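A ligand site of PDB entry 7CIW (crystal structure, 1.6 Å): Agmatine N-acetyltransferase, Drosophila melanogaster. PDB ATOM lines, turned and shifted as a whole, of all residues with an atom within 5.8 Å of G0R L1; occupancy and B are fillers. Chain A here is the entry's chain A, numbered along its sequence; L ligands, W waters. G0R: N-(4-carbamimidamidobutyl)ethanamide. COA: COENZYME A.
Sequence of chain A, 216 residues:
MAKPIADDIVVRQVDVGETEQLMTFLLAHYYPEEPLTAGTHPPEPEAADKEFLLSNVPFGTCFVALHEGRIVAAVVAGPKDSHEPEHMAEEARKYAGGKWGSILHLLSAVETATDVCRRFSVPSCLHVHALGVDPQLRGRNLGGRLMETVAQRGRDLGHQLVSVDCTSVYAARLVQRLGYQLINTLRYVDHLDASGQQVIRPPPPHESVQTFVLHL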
ATOM      1  N   TYR A  30      34.558   6.610   5.115  1.00  0.00           N
ATOM      2  CA  TYR A  30      33.804   7.582   5.898  1.00  0.00           C
ATOM      3  C   TYR A  30      33.713   7.143   7.349  1.00  0.00           C
ATOM      4  O   TYR A  30      34.260   7.817   8.239  1.00  0.00           O
ATOM      5  CB  TYR A  30      32.404   7.781   5.307  1.00  0.00           C
ATOM      6  CG  TYR A  30      31.503   8.621   6.190  1.00  0.00           C
ATOM      7  CD1 TYR A  30      31.684  10.002   6.280  1.00  0.00           C
ATOM      8  CD2 TYR A  30      30.469   8.043   6.917  1.00  0.00           C
ATOM      9  CE1 TYR A  30      30.869  10.772   7.085  1.00  0.00           C
ATOM     10  CE2 TYR A  30      29.643   8.809   7.731  1.00  0.00           C
ATOM     11  CZ  TYR A  30      29.857  10.177   7.799  1.00  0.00           C
ATOM     12  OH  TYR A  30      29.036  10.934   8.602  1.00  0.00           O
ATOM     13  N   TYR A  31      33.056   6.023   7.597  1.00  0.00           N
ATOM     14  CA  TYR A  31      32.801   5.585   8.963  1.00  0.00           C
ATOM     15  C   TYR A  31      34.061   5.365   9.811  1.00  0.00           C
ATOM     16  O   TYR A  31      34.030   5.707  11.000  1.00  0.00           O
ATOM     17  CB  TYR A  31      31.972   4.304   8.922  1.00  0.00           C
ATOM     18  CG  TYR A  31      30.483   4.474   8.725  1.00  0.00           C
ATOM     19  CD1 TYR A  31      29.697   5.101   9.688  1.00  0.00           C
ATOM     20  CD2 TYR A  31      29.858   3.943   7.611  1.00  0.00           C
ATOM     21  CE1 TYR A  31      28.312   5.210   9.528  1.00  0.00           C
ATOM     22  CE2 TYR A  31      28.476   4.034   7.448  1.00  0.00           C
ATOM     23  CZ  TYR A  31      27.712   4.659   8.414  1.00  0.00           C
ATOM     24  OH  TYR A  31      26.350   4.740   8.260  1.00  0.00           O
ATOM     25  N   GLU A  34      35.143   9.075  10.726  1.00  0.00           N
ATOM     26  CA  GLU A  34      34.159  10.042  11.201  1.00  0.00           C
ATOM     27  C   GLU A  34      34.180  10.076  12.724  1.00  0.00           C
ATOM     28  O   GLU A  34      34.089   9.020  13.367  1.00  0.00           O
ATOM     29  CB  GLU A  34      32.772   9.678  10.676  1.00  0.00           C
ATOM     30  CG  GLU A  34      31.752  10.780  10.883  1.00  0.00           C
ATOM     31  CD  GLU A  34      31.203  10.773  12.287  1.00  0.00           C
ATOM     32  OE1 GLU A  34      30.833   9.679  12.760  1.00  0.00           O
ATOM     33  OE2 GLU A  34      31.175  11.847  12.925  1.00  0.00           O
ATOM     34  N   LEU A  36      32.210  10.758  15.408  1.00  0.00           N
ATOM     35  CA  LEU A  36      31.246  10.058  16.284  1.00  0.00           C
ATOM     36  C   LEU A  36      31.368   8.550  16.147  1.00  0.00           C
ATOM     37  O   LEU A  36      31.277   7.822  17.134  1.00  0.00           O
ATOM     38  CB  LEU A  36      29.809  10.475  15.987  1.00  0.00           C
ATOM     39  CG  LEU A  36      29.505  11.966  15.995  1.00  0.00           C
ATOM     40  CD1 LEU A  36      27.983  12.165  15.939  1.00  0.00           C
ATOM     41  CD2 LEU A  36      30.111  12.616  17.236  1.00  0.00           C
ATOM     42  N   THR A  37      31.538   8.062  14.916  1.00  0.00           N
ATOM     43  CA  THR A  37      31.695   6.635  14.680  1.00  0.00           C
ATOM     44  C   THR A  37      33.000   6.120  15.268  1.00  0.00           C
ATOM     45  O   THR A  37      33.035   5.041  15.873  1.00  0.00           O
ATOM     46  CB  THR A  37      31.614   6.351  13.183  1.00  0.00           C
ATOM     47  OG1 THR A  37      30.554   7.135  12.616  1.00  0.00           O
ATOM     48  CG2 THR A  37      31.332   4.882  12.917  1.00  0.00           C
ATOM     49  N   PRO A  45      29.586   0.613  12.117  1.00  0.00           N
ATOM     50  CA  PRO A  45      28.239   1.127  12.415  1.00  0.00           C
ATOM     51  C   PRO A  45      27.196   0.023  12.461  1.00  0.00           C
ATOM     52  O   PRO A  45      27.304  -1.006  11.792  1.00  0.00           O
ATOM     53  CB  PRO A  45      27.969   2.093  11.249  1.00  0.00           C
ATOM     54  CG  PRO A  45      28.843   1.590  10.144  1.00  0.00           C
ATOM     55  CD  PRO A  45      30.097   1.111  10.827  1.00  0.00           C
ATOM     56  N   ASP A  49      22.075   2.560  11.768  1.00  0.00           N
ATOM     57  CA  ASP A  49      22.908   3.690  11.343  1.00  0.00           C
ATOM     58  C   ASP A  49      23.048   3.714   9.828  1.00  0.00           C
ATOM     59  O   ASP A  49      22.710   4.698   9.156  1.00  0.00           O
ATOM     60  CB  ASP A  49      24.266   3.569  12.035  1.00  0.00           C
ATOM     61  CG  ASP A  49      25.205   4.747  11.785  1.00  0.00           C
ATOM     62  OD1 ASP A  49      25.088   5.451  10.765  1.00  0.00           O
ATOM     63  OD2 ASP A  49      26.120   4.931  12.637  1.00  0.00           O
ATOM     64  N   PHE A  52      19.728   4.386   8.055  1.00  0.00           N
ATOM     65  CA  PHE A  52      19.286   5.771   8.049  1.00  0.00           C
ATOM     66  C   PHE A  52      19.979   6.563   6.940  1.00  0.00           C
ATOM     67  O   PHE A  52      19.333   7.328   6.221  1.00  0.00           O
ATOM     68  CB  PHE A  52      19.550   6.461   9.378  1.00  0.00           C
ATOM     69  CG  PHE A  52      19.397   7.940   9.289  1.00  0.00           C
ATOM     70  CD1 PHE A  52      18.154   8.493   8.996  1.00  0.00           C
ATOM     71  CD2 PHE A  52      20.484   8.786   9.390  1.00  0.00           C
ATOM     72  CE1 PHE A  52      17.985   9.860   8.859  1.00  0.00           C
ATOM     73  CE2 PHE A  52      20.330  10.162   9.252  1.00  0.00           C
ATOM     74  CZ  PHE A  52      19.071  10.688   8.986  1.00  0.00           C
ATOM     75  N   LEU A  53      21.293   6.397   6.809  1.00  0.00           N
ATOM     76  CA  LEU A  53      21.980   7.087   5.718  1.00  0.00           C
ATOM     77  C   LEU A  53      21.345   6.729   4.377  1.00  0.00           C
ATOM     78  O   LEU A  53      21.028   7.602   3.571  1.00  0.00           O
ATOM     79  CB  LEU A  53      23.474   6.750   5.723  1.00  0.00           C
ATOM     80  CG  LEU A  53      24.289   7.447   6.811  1.00  0.00           C
ATOM     81  CD1 LEU A  53      25.783   7.342   6.519  1.00  0.00           C
ATOM     82  CD2 LEU A  53      23.868   8.906   6.954  1.00  0.00           C
ATOM     83  N   TRP A 100      24.483   3.185  17.698  1.00  0.00           N
ATOM     84  CA  TRP A 100      23.628   4.160  17.028  1.00  0.00           C
ATOM     85  C   TRP A 100      22.888   5.019  18.035  1.00  0.00           C
ATOM     86  O   TRP A 100      22.738   6.236  17.830  1.00  0.00           O
ATOM     87  CB  TRP A 100      22.652   3.415  16.107  1.00  0.00           C
ATOM     88  CG  TRP A 100      21.710   4.232  15.260  1.00  0.00           C
ATOM     89  CD1 TRP A 100      20.385   3.987  15.068  1.00  0.00           C
ATOM     90  CD2 TRP A 100      22.029   5.380  14.464  1.00  0.00           C
ATOM     91  NE1 TRP A 100      19.846   4.915  14.212  1.00  0.00           N
ATOM     92  CE2 TRP A 100      20.837   5.780  13.814  1.00  0.00           C
ATOM     93  CE3 TRP A 100      23.196   6.105  14.225  1.00  0.00           C
ATOM     94  CZ2 TRP A 100      20.779   6.882  12.970  1.00  0.00           C
ATOM     95  CZ3 TRP A 100      23.130   7.187  13.385  1.00  0.00           C
ATOM     96  CH2 TRP A 100      21.936   7.568  12.762  1.00  0.00           C
ATOM     97  N   ILE A 103      25.259   7.719  19.207  1.00  0.00           N
ATOM     98  CA  ILE A 103      25.449   8.708  18.153  1.00  0.00           C
ATOM     99  C   ILE A 103      24.194   9.563  18.006  1.00  0.00           C
ATOM    100  O   ILE A 103      24.272  10.799  17.931  1.00  0.00           O
ATOM    101  CB  ILE A 103      25.837   7.995  16.839  1.00  0.00           C
ATOM    102  CG1 ILE A 103      27.192   7.289  16.992  1.00  0.00           C
ATOM    103  CG2 ILE A 103      25.807   8.960  15.653  1.00  0.00           C
ATOM    104  CD1 ILE A 103      27.652   6.514  15.773  1.00  0.00           C
ATOM    105  N   LEU A 107      23.574  13.647  18.241  1.00  0.00           N
ATOM    106  CA  LEU A 107      22.983  14.373  17.114  1.00  0.00           C
ATOM    107  C   LEU A 107      21.660  15.023  17.492  1.00  0.00           C
ATOM    108  O   LEU A 107      21.328  16.123  17.015  1.00  0.00           O
ATOM    109  CB  LEU A 107      22.805  13.422  15.927  1.00  0.00           C
ATOM    110  CG  LEU A 107      24.113  12.984  15.272  1.00  0.00           C
ATOM    111  CD1 LEU A 107      23.842  11.956  14.171  1.00  0.00           C
ATOM    112  CD2 LEU A 107      24.874  14.172  14.715  1.00  0.00           C
ATOM    113  N   VAL A 128      22.964  17.974   5.632  1.00  0.00           N
ATOM    114  CA  VAL A 128      23.992  17.057   5.153  1.00  0.00           C
ATOM    115  C   VAL A 128      24.323  16.077   6.271  1.00  0.00           C
ATOM    116  O   VAL A 128      24.877  16.462   7.309  1.00  0.00           O
ATOM    117  CB  VAL A 128      25.240  17.811   4.682  1.00  0.00           C
ATOM    118  CG1 VAL A 128      26.352  16.827   4.308  1.00  0.00           C
ATOM    119  CG2 VAL A 128      24.881  18.710   3.502  1.00  0.00           C
ATOM    120  N   HIS A 129      23.952  14.797   6.083  1.00  0.00           N
ATOM    121  CA  HIS A 129      24.135  13.752   7.071  1.00  0.00           C
ATOM    122  C   HIS A 129      25.496  13.069   7.009  1.00  0.00           C
ATOM    123  O   HIS A 129      25.940  12.527   8.026  1.00  0.00           O
ATOM    124  CB  HIS A 129      23.031  12.683   6.930  1.00  0.00           C
ATOM    125  CG  HIS A 129      21.671  13.190   7.279  1.00  0.00           C
ATOM    126  ND1 HIS A 129      21.308  13.519   8.559  1.00  0.00           N
ATOM    127  CD2 HIS A 129      20.584  13.437   6.505  1.00  0.00           C
ATOM    128  CE1 HIS A 129      20.054  13.938   8.570  1.00  0.00           C
ATOM    129  NE2 HIS A 129      19.596  13.909   7.324  1.00  0.00           N
ATOM    130  N   ALA A 130      26.164  13.084   5.865  1.00  0.00           N
ATOM    131  CA  ALA A 130      27.459  12.420   5.773  1.00  0.00           C
ATOM    132  C   ALA A 130      28.244  12.996   4.602  1.00  0.00           C
ATOM    133  O   ALA A 130      27.666  13.320   3.564  1.00  0.00           O
ATOM    134  CB  ALA A 130      27.290  10.911   5.591  1.00  0.00           C
ATOM    135  N   LEU A 131      29.548  13.163   4.804  1.00  0.00           N
ATOM    136  CA  LEU A 131      30.475  13.632   3.774  1.00  0.00           C
ATOM    137  C   LEU A 131      31.793  12.899   3.963  1.00  0.00           C
ATOM    138  O   LEU A 131      32.375  12.969   5.039  1.00  0.00           O
ATOM    139  CB  LEU A 131      30.680  15.142   3.870  1.00  0.00           C
ATOM    140  CG  LEU A 131      31.599  15.713   2.802  1.00  0.00           C
ATOM    141  CD1 LEU A 131      30.904  15.706   1.457  1.00  0.00           C
ATOM    142  CD2 LEU A 131      32.005  17.140   3.202  1.00  0.00           C
ATOM    143  N   VAL A 164      24.712  21.509   8.409  1.00  0.00           N
ATOM    144  CA  VAL A 164      25.632  20.379   8.494  1.00  0.00           C
ATOM    145  C   VAL A 164      26.301  20.363   9.868  1.00  0.00           C
ATOM    146  O   VAL A 164      26.729  21.407  10.367  1.00  0.00           O
ATOM    147  CB  VAL A 164      26.657  20.424   7.340  1.00  0.00           C
ATOM    148  CG1 VAL A 164      27.457  21.751   7.364  1.00  0.00           C
ATOM    149  CG2 VAL A 164      27.596  19.212   7.377  1.00  0.00           C
ATOM    150  N   ASP A 165      26.348  19.187  10.518  1.00  0.00           N
ATOM    151  CA  ASP A 165      27.036  19.033  11.805  1.00  0.00           C
ATOM    152  C   ASP A 165      28.464  18.587  11.538  1.00  0.00           C
ATOM    153  O   ASP A 165      28.721  17.412  11.305  1.00  0.00           O
ATOM    154  CB  ASP A 165      26.331  18.022  12.699  1.00  0.00           C
ATOM    155  CG  ASP A 165      24.891  18.375  12.995  1.00  0.00           C
ATOM    156  OD1 ASP A 165      24.586  19.582  13.153  1.00  0.00           O
ATOM    157  OD2 ASP A 165      24.059  17.449  13.088  1.00  0.00           O
ATOM    158  N   CYS A 166      29.404  19.522  11.605  1.00  0.00           N
ATOM    159  CA  CYS A 166      30.811  19.182  11.383  1.00  0.00           C
ATOM    160  C   CYS A 166      31.385  18.595  12.662  1.00  0.00           C
ATOM    161  O   CYS A 166      31.887  19.298  13.544  1.00  0.00           O
ATOM    162  CB  CYS A 166      31.586  20.408  10.912  1.00  0.00           C
ATOM    163  SG  CYS A 166      31.036  21.024   9.299  1.00  0.00           S
ATOM    164  N   THR A 167      31.281  17.279  12.777  1.00  0.00           N
ATOM    165  CA  THR A 167      31.907  16.558  13.857  1.00  0.00           C
ATOM    166  C   THR A 167      33.429  16.540  13.715  1.00  0.00           C
ATOM    167  O   THR A 167      34.134  16.327  14.704  1.00  0.00           O
ATOM    168  CB  THR A 167      31.357  15.130  13.900  1.00  0.00           C
ATOM    169  OG1 THR A 167      31.606  14.506  12.639  1.00  0.00           O
ATOM    170  CG2 THR A 167      29.850  15.162  14.129  1.00  0.00           C
HETATM  171  C10 G0R L   1      26.456   8.542  11.535  1.00  0.00           C
HETATM  172  N12 G0R L   1      27.435   7.711  12.228  1.00  0.00           N
HETATM  173  C1  G0R L   1      28.573  15.639   7.376  1.00  0.00           C
HETATM  174  C2  G0R L   1      28.876  14.542   8.402  1.00  0.00           C
HETATM  175  C5  G0R L   1      28.664  13.695  10.775  1.00  0.00           C
HETATM  176  C6  G0R L   1      27.408  12.851  11.048  1.00  0.00           C
HETATM  177  C7  G0R L   1      27.576  11.913  12.249  1.00  0.00           C
HETATM  178  C8  G0R L   1      27.807  10.434  11.905  1.00  0.00           C
HETATM  179  N4  G0R L   1      28.406  14.706   9.769  1.00  0.00           N
HETATM  180  N9  G0R L   1      26.621   9.777  11.403  1.00  0.00           N
HETATM  181  N11 G0R L   1      25.263   7.939  11.001  1.00  0.00           N
HETATM  182  O3  G0R L   1      29.474  13.578   8.087  1.00  0.00           O
HETATM  183  N1A COA L   2      43.032  14.213   7.819  1.00  0.00           N
HETATM  184  C2A COA L   2      44.142  14.993   7.664  1.00  0.00           C
HETATM  185  N3A COA L   2      44.126  16.057   6.785  1.00  0.00           N
HETATM  186  C4A COA L   2      43.028  16.326   6.068  1.00  0.00           C
HETATM  187  C5A COA L   2      41.942  15.551   6.220  1.00  0.00           C
HETATM  188  C6A COA L   2      41.962  14.493   7.107  1.00  0.00           C
HETATM  189  N6A COA L   2      41.039  13.395   7.610  1.00  0.00           N
HETATM  190  N7A COA L   2      40.956  16.000   5.404  1.00  0.00           N
HETATM  191  C8A COA L   2      41.424  17.064   4.730  1.00  0.00           C
HETATM  192  N9A COA L   2      42.678  17.260   5.148  1.00  0.00           N
HETATM  193  C1B COA L   2      43.650  18.126   4.812  1.00  0.00           C
HETATM  194  C2B COA L   2      43.921  17.917   3.292  1.00  0.00           C
HETATM  195  O2B COA L   2      44.857  16.795   3.049  1.00  0.00           O
HETATM  196  C3B COA L   2      44.351  19.113   2.837  1.00  0.00           C
HETATM  197  O3B COA L   2      45.711  19.459   3.232  1.00  0.00           O
HETATM  198  P3B COA L   2      47.045  19.154   2.293  1.00  0.00           P
HETATM  199  O7A COA L   2      46.678  19.197   0.821  1.00  0.00           O
HETATM  200  O8A COA L   2      48.165  20.142   2.649  1.00  0.00           O
HETATM  201  O9A COA L   2      47.484  17.741   2.672  1.00  0.00           O
HETATM  202  C4B COA L   2      43.456  20.191   3.677  1.00  0.00           C
HETATM  203  O4B COA L   2      43.116  19.599   4.822  1.00  0.00           O
HETATM  204  C5B COA L   2      42.262  20.655   2.894  1.00  0.00           C
HETATM  205  O5B COA L   2      41.674  19.521   2.264  1.00  0.00           O
HETATM  206  P1A COA L   2      40.081  19.551   1.743  1.00  0.00           P
HETATM  207  O1A COA L   2      39.273  20.705   2.329  1.00  0.00           O
HETATM  208  O2A COA L   2      40.058  19.510   0.225  1.00  0.00           O
HETATM  209  O3A COA L   2      39.453  18.167   2.373  1.00  0.00           O
HETATM  210  P2A COA L   2      38.587  17.028   1.565  1.00  0.00           P
HETATM  211  O4A COA L   2      39.462  16.305   0.592  1.00  0.00           O
HETATM  212  O5A COA L   2      37.367  17.658   0.934  1.00  0.00           O
HETATM  213  O6A COA L   2      38.195  16.031   2.823  1.00  0.00           O
HETATM  214  CBP COA L   2      36.711  15.384   4.484  1.00  0.00           C
HETATM  215  CCP COA L   2      37.463  16.551   3.881  1.00  0.00           C
HETATM  216  CDP COA L   2      35.612  14.955   3.445  1.00  0.00           C
HETATM  217  CEP COA L   2      36.061  15.803   5.802  1.00  0.00           C
HETATM  218  CAP COA L   2      37.715  14.270   4.763  1.00  0.00           C
HETATM  219  OAP COA L   2      38.583  14.691   5.784  1.00  0.00           O
HETATM  220  C9P COA L   2      37.075  12.939   5.195  1.00  0.00           C
HETATM  221  O9P COA L   2      36.549  12.193   4.433  1.00  0.00           O
HETATM  222  N8P COA L   2      37.156  12.581   6.606  1.00  0.00           N
HETATM  223  C7P COA L   2      36.621  11.303   7.104  1.00  0.00           C
HETATM  224  C6P COA L   2      35.048  11.261   7.286  1.00  0.00           C
HETATM  225  C5P COA L   2      34.669  12.507   8.059  1.00  0.00           C
HETATM  226  O5P COA L   2      35.171  12.789   9.114  1.00  0.00           O
HETATM  227  N4P COA L   2      33.637  13.373   7.409  1.00  0.00           N
HETATM  228  C3P COA L   2      33.178  14.637   7.950  1.00  0.00           C
HETATM  229  C2P COA L   2      32.385  14.481   9.253  1.00  0.00           C
HETATM  230  S1P COA L   2      31.779  16.180   9.491  1.00  0.00           S
HETATM  231  O   HOH W   1      24.500  11.072  10.109  1.00  0.00           O
HETATM  232  O   HOH W   2      26.013  16.380   9.714  1.00  0.00           O
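Water W1 bridges a nitrogen (N9) of G0R L1 (2.8 Å) and the backbone carbonyl oxygen (O) of His 129 (2.9 Å). Water W2 lies within hydrogen-bond range of the backbone carbonyl oxygen of Val 128 (2.7 Å), a nitrogen (N4) of G0R L1 (2.9 Å) and the backbone NH of Asp 165 (2.9 Å).
Tyr 31 touches G0R L1 (CE1 to N12, 3.8 Å). Leu 36 touches G0R L1 (CD1 to C7, 3.7 Å). CZ3 of Trp 100 touches N11 of G0R L1, 3.3 Å away. Ile 103 touches G0R L1. O of Val 128 touches C1 of G0R L1, 3.8 Å away. His 129 touches G0R L1 (O to C6, 3.4 Å). Ala 130 touches G0R L1. CG2 of Val 164 touches C1 of G0R L1, 3.7 Å away. OG1 of Thr 167 touches C5 of G0R L1, at 3.6 Å. Within 4 Å of G0R L1: Tyr 30, Tyr 31, Glu 34, Leu 36, Thr 37, Asp 49, Trp 100, Ile 103, Val 128, His 129, Ala 130, Leu 131, Val 164, Asp 165 and Thr 167.
A nitrogen (N4) of G0R L1 lies close to a sulfur (S1P) of COA L2, at 3.7 Å.
The side-chain carboxylate (OD1) of Asp 49 lies within hydrogen-bond range of the side-chain hydroxyl (OH) of Tyr 31, at 2.9 Å. The side-chain carboxylate (OE1) of Glu 34 lies within hydrogen-bond range of the side-chain hydroxyl (OG1) of Thr 37, 2.6 Å away. OG1 of Thr 167 is in hydrogen-bond range of OE2 of Glu 34 (2.7 Å). N of Leu 36 lies within hydrogen-bond range of OE2 of Glu 34.
The side-chain carboxylate (OD1) of Asp 49 is in salt-bridge range of a nitrogen (N11) of G0R L1 (2.5 Å). The side-chain hydroxyl (OH) of Tyr 30 sits at hydrogen-bond distance from an oxygen (O3) of G0R L1 (2.7 Å). A nitrogen (N4) of G0R L1 sits at hydrogen-bond distance from the backbone carbonyl oxygen (O) of Asp 165, at 3.1 Å. OG1 of Thr 37 lies within hydrogen-bond range of N12 of G0R L1, 3.2 Å away. A nitrogen (N12) of G0R L1 is in salt-bridge range of the side-chain carboxylate (OE1) of Glu 34, at 3.96 Å. The backbone NH of Leu 131 is in hydrogen-bond range of an oxygen (O3) of G0R L1 (3.3 Å). S1P of COA L2 lies close to O of Asp 165 (3.8 Å). O of Leu 131 is in hydrogen-bond range of N4P of COA L2, 2.7 Å away. The backbone NH (N) of Thr 167 sits close to a sulfur (S1P) of COA L2, at 3.5 Å. OG1 of Thr 167 lies close to S1P of COA L2, at 3.6 Å.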
